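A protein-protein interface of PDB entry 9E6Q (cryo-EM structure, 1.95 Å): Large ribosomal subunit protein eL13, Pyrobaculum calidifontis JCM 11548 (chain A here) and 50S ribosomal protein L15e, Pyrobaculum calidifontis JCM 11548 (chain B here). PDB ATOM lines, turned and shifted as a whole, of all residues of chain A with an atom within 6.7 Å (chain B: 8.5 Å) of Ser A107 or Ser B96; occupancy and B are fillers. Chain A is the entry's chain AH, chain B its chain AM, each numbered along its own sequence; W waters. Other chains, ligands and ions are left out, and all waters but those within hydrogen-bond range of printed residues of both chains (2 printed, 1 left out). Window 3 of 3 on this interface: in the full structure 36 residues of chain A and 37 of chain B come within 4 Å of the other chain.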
ATOM      1  N   SER A 102      15.223  -6.103   8.309  1.00  0.00           N
ATOM      2  CA  SER A 102      13.859  -5.694   8.003  1.00  0.00           C
ATOM      3  C   SER A 102      12.856  -6.349   8.946  1.00  0.00           C
ATOM      4  O   SER A 102      11.884  -5.713   9.361  1.00  0.00           O
ATOM      5  CB  SER A 102      13.535  -6.020   6.549  1.00  0.00           C
ATOM      6  OG  SER A 102      12.682  -5.042   5.996  1.00  0.00           O
ATOM      7  N   ALA A 103      13.072  -7.619   9.296  1.00  0.00           N
ATOM      8  CA  ALA A 103      12.185  -8.279  10.246  1.00  0.00           C
ATOM      9  C   ALA A 103      12.227  -7.595  11.605  1.00  0.00           C
ATOM     10  O   ALA A 103      11.185  -7.368  12.224  1.00  0.00           O
ATOM     11  CB  ALA A 103      12.557  -9.751  10.379  1.00  0.00           C
ATOM     12  N   GLY A 104      13.422  -7.252  12.082  1.00  0.00           N
ATOM     13  CA  GLY A 104      13.523  -6.531  13.335  1.00  0.00           C
ATOM     14  C   GLY A 104      12.893  -5.157  13.264  1.00  0.00           C
ATOM     15  O   GLY A 104      12.199  -4.737  14.189  1.00  0.00           O
ATOM     16  N   ARG A 105      13.105  -4.449  12.156  1.00  0.00           N
ATOM     17  CA  ARG A 105      12.531  -3.118  12.007  1.00  0.00           C
ATOM     18  C   ARG A 105      11.012  -3.167  12.030  1.00  0.00           C
ATOM     19  O   ARG A 105      10.367  -2.257  12.555  1.00  0.00           O
ATOM     20  CB  ARG A 105      13.023  -2.467  10.718  1.00  0.00           C
ATOM     21  CG  ARG A 105      14.378  -1.816  10.845  1.00  0.00           C
ATOM     22  CD  ARG A 105      14.838  -1.212   9.537  1.00  0.00           C
ATOM     23  NE  ARG A 105      13.763  -0.507   8.854  1.00  0.00           N
ATOM     24  CZ  ARG A 105      13.397   0.738   9.124  1.00  0.00           C
ATOM     25  NH1 ARG A 105      13.997   1.446  10.063  1.00  0.00           N
ATOM     26  NH2 ARG A 105      12.403   1.284   8.434  1.00  0.00           N
ATOM     27  N   ARG A 106      10.423  -4.212  11.451  1.00  0.00           N
ATOM     28  CA  ARG A 106       8.970  -4.342  11.472  1.00  0.00           C
ATOM     29  C   ARG A 106       8.457  -4.558  12.888  1.00  0.00           C
ATOM     30  O   ARG A 106       7.536  -3.874  13.332  1.00  0.00           O
ATOM     31  CB  ARG A 106       8.524  -5.484  10.567  1.00  0.00           C
ATOM     32  CG  ARG A 106       7.030  -5.675  10.559  1.00  0.00           C
ATOM     33  CD  ARG A 106       6.627  -6.862   9.728  1.00  0.00           C
ATOM     34  NE  ARG A 106       6.919  -6.681   8.312  1.00  0.00           N
ATOM     35  CZ  ARG A 106       6.226  -5.912   7.487  1.00  0.00           C
ATOM     36  NH1 ARG A 106       5.184  -5.216   7.903  1.00  0.00           N
ATOM     37  NH2 ARG A 106       6.588  -5.840   6.214  1.00  0.00           N
ATOM     38  N   SER A 107       9.052  -5.502  13.617  1.00  0.00           N
ATOM     39  CA  SER A 107       8.595  -5.786  14.970  1.00  0.00           C
ATOM     40  C   SER A 107       8.774  -4.590  15.891  1.00  0.00           C
ATOM     41  O   SER A 107       7.969  -4.394  16.805  1.00  0.00           O
ATOM     42  CB  SER A 107       9.328  -6.997  15.533  1.00  0.00           C
ATOM     43  OG  SER A 107       9.076  -8.139  14.746  1.00  0.00           O
ATOM     44  N   ARG A 108       9.812  -3.787  15.674  1.00  0.00           N
ATOM     45  CA  ARG A 108      10.010  -2.587  16.475  1.00  0.00           C
ATOM     46  C   ARG A 108       9.012  -1.489  16.147  1.00  0.00           C
ATOM     47  O   ARG A 108       8.965  -0.491  16.866  1.00  0.00           O
ATOM     48  CB  ARG A 108      11.427  -2.049  16.294  1.00  0.00           C
ATOM     49  CG  ARG A 108      12.507  -2.962  16.816  1.00  0.00           C
ATOM     50  CD  ARG A 108      13.852  -2.612  16.236  1.00  0.00           C
ATOM     51  NE  ARG A 108      14.360  -1.346  16.743  1.00  0.00           N
ATOM     52  CZ  ARG A 108      15.306  -0.634  16.152  1.00  0.00           C
ATOM     53  NH1 ARG A 108      15.854  -1.024  15.019  1.00  0.00           N
ATOM     54  NH2 ARG A 108      15.713   0.497  16.715  1.00  0.00           N
ATOM     55  N   GLY A 109       8.220  -1.644  15.094  1.00  0.00           N
ATOM     56  CA  GLY A 109       7.230  -0.665  14.725  1.00  0.00           C
ATOM     57  C   GLY A 109       7.696   0.378  13.739  1.00  0.00           C
ATOM     58  O   GLY A 109       6.915   1.269  13.395  1.00  0.00           O
ATOM     59  N   LEU A 110       8.930   0.286  13.257  1.00  0.00           N
ATOM     60  CA  LEU A 110       9.522   1.326  12.430  1.00  0.00           C
ATOM     61  C   LEU A 110       9.020   1.323  10.998  1.00  0.00           C
ATOM     62  O   LEU A 110       9.323   2.260  10.256  1.00  0.00           O
ATOM     63  CB  LEU A 110      11.040   1.189  12.438  1.00  0.00           C
ATOM     64  CG  LEU A 110      11.647   1.622  13.765  1.00  0.00           C
ATOM     65  CD1 LEU A 110      12.997   0.990  13.982  1.00  0.00           C
ATOM     66  CD2 LEU A 110      11.740   3.128  13.800  1.00  0.00           C
ATOM     67  N   ILE A 111       8.278   0.303  10.585  1.00  0.00           N
ATOM     68  CA  ILE A 111       7.718   0.305   9.243  1.00  0.00           C
ATOM     69  C   ILE A 111       6.372   1.013   9.229  1.00  0.00           C
ATOM     70  O   ILE A 111       6.047   1.734   8.282  1.00  0.00           O
ATOM     71  CB  ILE A 111       7.624  -1.136   8.708  1.00  0.00           C
ATOM     72  CG1 ILE A 111       9.022  -1.652   8.369  1.00  0.00           C
ATOM     73  CG2 ILE A 111       6.722  -1.213   7.496  1.00  0.00           C
ATOM     74  CD1 ILE A 111       9.051  -3.035   7.806  1.00  0.00           C
ATOM     75  N   LEU B  67      11.819 -24.072  11.099  1.00  0.00           N
ATOM     76  CA  LEU B  67      11.532 -23.960  12.517  1.00  0.00           C
ATOM     77  C   LEU B  67      10.059 -24.230  12.772  1.00  0.00           C
ATOM     78  O   LEU B  67       9.217 -24.084  11.889  1.00  0.00           O
ATOM     79  CB  LEU B  67      11.934 -22.586  13.063  1.00  0.00           C
ATOM     80  CG  LEU B  67      11.579 -21.329  12.279  1.00  0.00           C
ATOM     81  CD1 LEU B  67      10.151 -20.917  12.557  1.00  0.00           C
ATOM     82  CD2 LEU B  67      12.525 -20.224  12.661  1.00  0.00           C
ATOM     83  N   GLY B  70       3.867 -21.363  15.389  1.00  0.00           N
ATOM     84  CA  GLY B  70       3.032 -21.202  16.549  1.00  0.00           C
ATOM     85  C   GLY B  70       3.623 -20.195  17.505  1.00  0.00           C
ATOM     86  O   GLY B  70       4.629 -19.552  17.216  1.00  0.00           O
ATOM     87  N   THR B  92       2.530 -14.495  23.139  1.00  0.00           N
ATOM     88  CA  THR B  92       3.537 -14.666  22.110  1.00  0.00           C
ATOM     89  C   THR B  92       4.729 -13.767  22.404  1.00  0.00           C
ATOM     90  O   THR B  92       4.729 -12.984  23.350  1.00  0.00           O
ATOM     91  CB  THR B  92       2.954 -14.356  20.731  1.00  0.00           C
ATOM     92  OG1 THR B  92       2.674 -12.958  20.645  1.00  0.00           O
ATOM     93  CG2 THR B  92       1.673 -15.124  20.505  1.00  0.00           C
ATOM     94  N   ALA B  93       5.748 -13.883  21.569  1.00  0.00           N
ATOM     95  CA  ALA B  93       6.946 -13.072  21.681  1.00  0.00           C
ATOM     96  C   ALA B  93       6.843 -11.854  20.775  1.00  0.00           C
ATOM     97  O   ALA B  93       6.173 -11.885  19.745  1.00  0.00           O
ATOM     98  CB  ALA B  93       8.184 -13.891  21.323  1.00  0.00           C
ATOM     99  N   TRP B  94       7.513 -10.775  21.170  1.00  0.00           N
ATOM    100  CA  TRP B  94       7.582  -9.598  20.314  1.00  0.00           C
ATOM    101  C   TRP B  94       8.524  -9.794  19.131  1.00  0.00           C
ATOM    102  O   TRP B  94       8.627  -8.898  18.294  1.00  0.00           O
ATOM    103  CB  TRP B  94       7.985  -8.370  21.133  1.00  0.00           C
ATOM    104  CG  TRP B  94       6.845  -7.795  21.949  1.00  0.00           C
ATOM    105  CD1 TRP B  94       5.724  -8.447  22.345  1.00  0.00           C
ATOM    106  CD2 TRP B  94       6.725  -6.459  22.449  1.00  0.00           C
ATOM    107  NE1 TRP B  94       4.912  -7.611  23.060  1.00  0.00           N
ATOM    108  CE2 TRP B  94       5.505  -6.383  23.141  1.00  0.00           C
ATOM    109  CE3 TRP B  94       7.532  -5.326  22.386  1.00  0.00           C
ATOM    110  CZ2 TRP B  94       5.074  -5.219  23.759  1.00  0.00           C
ATOM    111  CZ3 TRP B  94       7.101  -4.175  23.003  1.00  0.00           C
ATOM    112  CH2 TRP B  94       5.883  -4.127  23.673  1.00  0.00           C
ATOM    113  N   LYS B  95       9.217 -10.925  19.054  1.00  0.00           N
ATOM    114  CA  LYS B  95       9.997 -11.308  17.885  1.00  0.00           C
ATOM    115  C   LYS B  95       9.156 -12.144  16.931  1.00  0.00           C
ATOM    116  O   LYS B  95       8.409 -13.023  17.358  1.00  0.00           O
ATOM    117  CB  LYS B  95      11.220 -12.127  18.294  1.00  0.00           C
ATOM    118  CG  LYS B  95      12.509 -11.383  18.316  1.00  0.00           C
ATOM    119  CD  LYS B  95      13.669 -12.299  18.624  1.00  0.00           C
ATOM    120  CE  LYS B  95      14.876 -11.485  19.008  1.00  0.00           C
ATOM    121  NZ  LYS B  95      15.939 -12.297  19.627  1.00  0.00           N
ATOM    122  N   SER B  96       9.304 -11.882  15.639  1.00  0.00           N
ATOM    123  CA  SER B  96       8.718 -12.738  14.621  1.00  0.00           C
ATOM    124  C   SER B  96       9.592 -13.964  14.391  1.00  0.00           C
ATOM    125  O   SER B  96      10.777 -13.975  14.714  1.00  0.00           O
ATOM    126  CB  SER B  96       8.552 -11.976  13.312  1.00  0.00           C
ATOM    127  OG  SER B  96       9.810 -11.653  12.767  1.00  0.00           O
ATOM    128  N   TRP B  97       8.995 -15.005  13.809  1.00  0.00           N
ATOM    129  CA  TRP B  97       9.776 -16.193  13.486  1.00  0.00           C
ATOM    130  C   TRP B  97      10.808 -15.916  12.410  1.00  0.00           C
ATOM    131  O   TRP B  97      11.806 -16.631  12.334  1.00  0.00           O
ATOM    132  CB  TRP B  97       8.877 -17.349  13.046  1.00  0.00           C
ATOM    133  CG  TRP B  97       8.096 -17.957  14.157  1.00  0.00           C
ATOM    134  CD1 TRP B  97       6.770 -18.236  14.158  1.00  0.00           C
ATOM    135  CD2 TRP B  97       8.592 -18.373  15.432  1.00  0.00           C
ATOM    136  NE1 TRP B  97       6.401 -18.787  15.350  1.00  0.00           N
ATOM    137  CE2 TRP B  97       7.504 -18.882  16.152  1.00  0.00           C
ATOM    138  CE3 TRP B  97       9.850 -18.357  16.036  1.00  0.00           C
ATOM    139  CZ2 TRP B  97       7.632 -19.370  17.444  1.00  0.00           C
ATOM    140  CZ3 TRP B  97       9.970 -18.840  17.318  1.00  0.00           C
ATOM    141  CH2 TRP B  97       8.867 -19.335  18.010  1.00  0.00           C
ATOM    142  N   ARG B  98      10.593 -14.892  11.584  1.00  0.00           N
ATOM    143  CA  ARG B  98      11.577 -14.535  10.572  1.00  0.00           C
ATOM    144  C   ARG B  98      12.867 -14.028  11.203  1.00  0.00           C
ATOM    145  O   ARG B  98      13.959 -14.382  10.755  1.00  0.00           O
ATOM    146  CB  ARG B  98      10.998 -13.493   9.624  1.00  0.00           C
ATOM    147  CG  ARG B  98      11.931 -13.129   8.492  1.00  0.00           C
ATOM    148  CD  ARG B  98      11.184 -12.883   7.213  1.00  0.00           C
ATOM    149  NE  ARG B  98      10.505 -11.597   7.234  1.00  0.00           N
ATOM    150  CZ  ARG B  98      11.075 -10.442   6.931  1.00  0.00           C
ATOM    151  NH1 ARG B  98      12.337 -10.375   6.550  1.00  0.00           N
ATOM    152  NH2 ARG B  98      10.357  -9.328   7.002  1.00  0.00           N
ATOM    153  N   GLN B  99      12.765 -13.193  12.236  1.00  0.00           N
ATOM    154  CA  GLN B  99      13.964 -12.756  12.940  1.00  0.00           C
ATOM    155  C   GLN B  99      14.639 -13.918  13.653  1.00  0.00           C
ATOM    156  O   GLN B  99      15.869 -13.999  13.690  1.00  0.00           O
ATOM    157  CB  GLN B  99      13.630 -11.648  13.934  1.00  0.00           C
ATOM    158  CG  GLN B  99      14.821 -10.782  14.293  1.00  0.00           C
ATOM    159  CD  GLN B  99      14.580  -9.921  15.509  1.00  0.00           C
ATOM    160  OE1 GLN B  99      13.461  -9.490  15.762  1.00  0.00           O
ATOM    161  NE2 GLN B  99      15.633  -9.657  16.265  1.00  0.00           N
ATOM    162  N   VAL B 100      13.848 -14.817  14.237  1.00  0.00           N
ATOM    163  CA  VAL B 100      14.414 -15.992  14.886  1.00  0.00           C
ATOM    164  C   VAL B 100      15.178 -16.838  13.880  1.00  0.00           C
ATOM    165  O   VAL B 100      16.244 -17.377  14.185  1.00  0.00           O
ATOM    166  CB  VAL B 100      13.311 -16.802  15.588  1.00  0.00           C
ATOM    167  CG1 VAL B 100      13.853 -18.126  16.078  1.00  0.00           C
ATOM    168  CG2 VAL B 100      12.733 -16.011  16.732  1.00  0.00           C
ATOM    169  N   ALA B 101      14.639 -16.975  12.669  1.00  0.00           N
ATOM    170  CA  ALA B 101      15.318 -17.738  11.629  1.00  0.00           C
ATOM    171  C   ALA B 101      16.646 -17.097  11.244  1.00  0.00           C
ATOM    172  O   ALA B 101      17.658 -17.786  11.099  1.00  0.00           O
ATOM    173  CB  ALA B 101      14.410 -17.877  10.410  1.00  0.00           C
ATOM    174  N   GLU B 102      16.663 -15.774  11.081  1.00  0.00           N
ATOM    175  CA  GLU B 102      17.903 -15.091  10.728  1.00  0.00           C
ATOM    176  C   GLU B 102      18.960 -15.291  11.797  1.00  0.00           C
ATOM    177  O   GLU B 102      20.141 -15.470  11.490  1.00  0.00           O
ATOM    178  CB  GLU B 102      17.653 -13.599  10.525  1.00  0.00           C
ATOM    179  CG  GLU B 102      16.634 -13.270   9.475  1.00  0.00           C
ATOM    180  CD  GLU B 102      16.257 -11.801   9.469  1.00  0.00           C
ATOM    181  OE1 GLU B 102      15.791 -11.307   8.426  1.00  0.00           O
ATOM    182  OE2 GLU B 102      16.422 -11.137  10.511  1.00  0.00           O
ATOM    183  N   GLU B 103      18.554 -15.246  13.061  1.00  0.00           N
ATOM    184  CA  GLU B 103      19.505 -15.381  14.149  1.00  0.00           C
ATOM    185  C   GLU B 103      20.073 -16.793  14.213  1.00  0.00           C
ATOM    186  O   GLU B 103      21.268 -16.974  14.463  1.00  0.00           O
ATOM    187  CB  GLU B 103      18.820 -15.001  15.454  1.00  0.00           C
ATOM    188  CG  GLU B 103      19.026 -13.566  15.838  1.00  0.00           C
ATOM    189  CD  GLU B 103      18.254 -13.180  17.074  1.00  0.00           C
ATOM    190  OE1 GLU B 103      17.314 -12.375  16.954  1.00  0.00           O
ATOM    191  OE2 GLU B 103      18.589 -13.674  18.166  1.00  0.00           O
ATOM    192  N   SER B 117      16.048 -11.716   4.674  1.00  0.00           N
ATOM    193  CA  SER B 117      15.424 -13.031   4.622  1.00  0.00           C
ATOM    194  C   SER B 117      14.011 -12.886   4.087  1.00  0.00           C
ATOM    195  O   SER B 117      13.453 -11.792   4.049  1.00  0.00           O
ATOM    196  CB  SER B 117      15.388 -13.710   5.994  1.00  0.00           C
ATOM    197  OG  SER B 117      14.834 -12.850   6.961  1.00  0.00           O
ATOM    198  N   ARG B 127       7.670 -23.736   9.553  1.00  0.00           N
ATOM    199  CA  ARG B 127       7.733 -22.603   8.647  1.00  0.00           C
ATOM    200  C   ARG B 127       9.137 -22.557   8.070  1.00  0.00           C
ATOM    201  O   ARG B 127      10.110 -22.807   8.782  1.00  0.00           O
ATOM    202  CB  ARG B 127       7.398 -21.295   9.360  1.00  0.00           C
ATOM    203  CG  ARG B 127       7.421 -20.066   8.475  1.00  0.00           C
ATOM    204  CD  ARG B 127       6.562 -18.955   9.043  1.00  0.00           C
ATOM    205  NE  ARG B 127       5.143 -19.244   8.907  1.00  0.00           N
ATOM    206  CZ  ARG B 127       4.200 -18.797   9.723  1.00  0.00           C
ATOM    207  NH1 ARG B 127       4.487 -18.017  10.750  1.00  0.00           N
ATOM    208  NH2 ARG B 127       2.938 -19.133   9.498  1.00  0.00           N
ATOM    209  N   PHE B 129      12.112 -20.458   5.950  1.00  0.00           N
ATOM    210  CA  PHE B 129      12.666 -19.187   5.529  1.00  0.00           C
ATOM    211  C   PHE B 129      13.971 -19.430   4.797  1.00  0.00           C
ATOM    212  O   PHE B 129      14.639 -20.443   4.996  1.00  0.00           O
ATOM    213  CB  PHE B 129      12.945 -18.254   6.710  1.00  0.00           C
ATOM    214  CG  PHE B 129      11.740 -17.892   7.500  1.00  0.00           C
ATOM    215  CD1 PHE B 129      10.931 -16.852   7.108  1.00  0.00           C
ATOM    216  CD2 PHE B 129      11.423 -18.580   8.648  1.00  0.00           C
ATOM    217  CE1 PHE B 129       9.831 -16.513   7.834  1.00  0.00           C
ATOM    218  CE2 PHE B 129      10.326 -18.238   9.379  1.00  0.00           C
ATOM    219  CZ  PHE B 129       9.531 -17.202   8.971  1.00  0.00           C
HETATM  220  O   HOH W   1       8.814  -8.927  11.683  1.00  0.00           O
HETATM  221  O   HOH W   2      11.180  -9.701  14.824  1.00  0.00           O
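Of chain B, only Trp B94 (3.4 Å) and Ser B96 (3.9 Å) come within 4 Å of Ser A107. Of chain A, only Ser A107 (3.9 Å) comes within 4 Å of Ser B96. Printed residues of chain A within 4 Å of Trp B94: Ser A107. Printed residues of chain A within 4 Å of Gln B99: Ala A103 and Gly A104. Lys B95 touches none of the printed residues of chain A. Val B100 touches none of the printed residues of chain A.
OG of Ser A107 lies within hydrogen-bond range of O of Ala A103 (3.4 Å). The side-chain hydroxyl (OG) of Ser B96 sits at hydrogen-bond distance from the backbone NH (N) of Gln B99, 3.4 Å away. O of Ser B117 is in hydrogen-bond range of NH1 of Arg B98, 3.1 Å away. The side-chain carboxylate (OE1) of Glu B103 is in hydrogen-bond range of the side-chain amide nitrogen (NE2) of Gln B99 (3.3 Å).
Water W2 lies within hydrogen-bond range of OE1 of Gln B99 (2.5 Å), OG of Ser A107 (2.6 Å), N of Ser B96 (3.0 Å) and O of Ala A103 (3.5 Å). Water W1 lies within hydrogen-bond range of O of Ala A103 (2.9 Å), OG of Ser B96 (3.1 Å) and OG of Ser A107 (3.2 Å).
Printed residues of chain A that touch a printed residue of chain B: Ala A103, Gly A104 and Ser A107. Of the 17 printed residues of chain B, 4 touch a printed residue of chain A. Printed residues of chain B that touch a printed residue of chain A: Trp B94, Ser B96, Arg B98 and Gln B99. Along chain B the printed residues that touch a printed residue of chain A span positions 94 to 99. Among the printed residues, 5 pairs touch across the chains. Among the printed residues, no Asp or Glu carboxylate lies within 4 Å of a Lys or Arg side-chain nitrogen of the other chain.
CB of Ala A103 touches CZ of Arg B98, 3.8 Å away. Gln B99 touches Ala A103 (N to CB, 3.9 Å). CA of Gly A104 touches OE1 of Gln B99, at 3.8 Å. Ser A107 touches Trp B94. OG of Ser A107 touches N of Ser B96 (3.9 Å).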
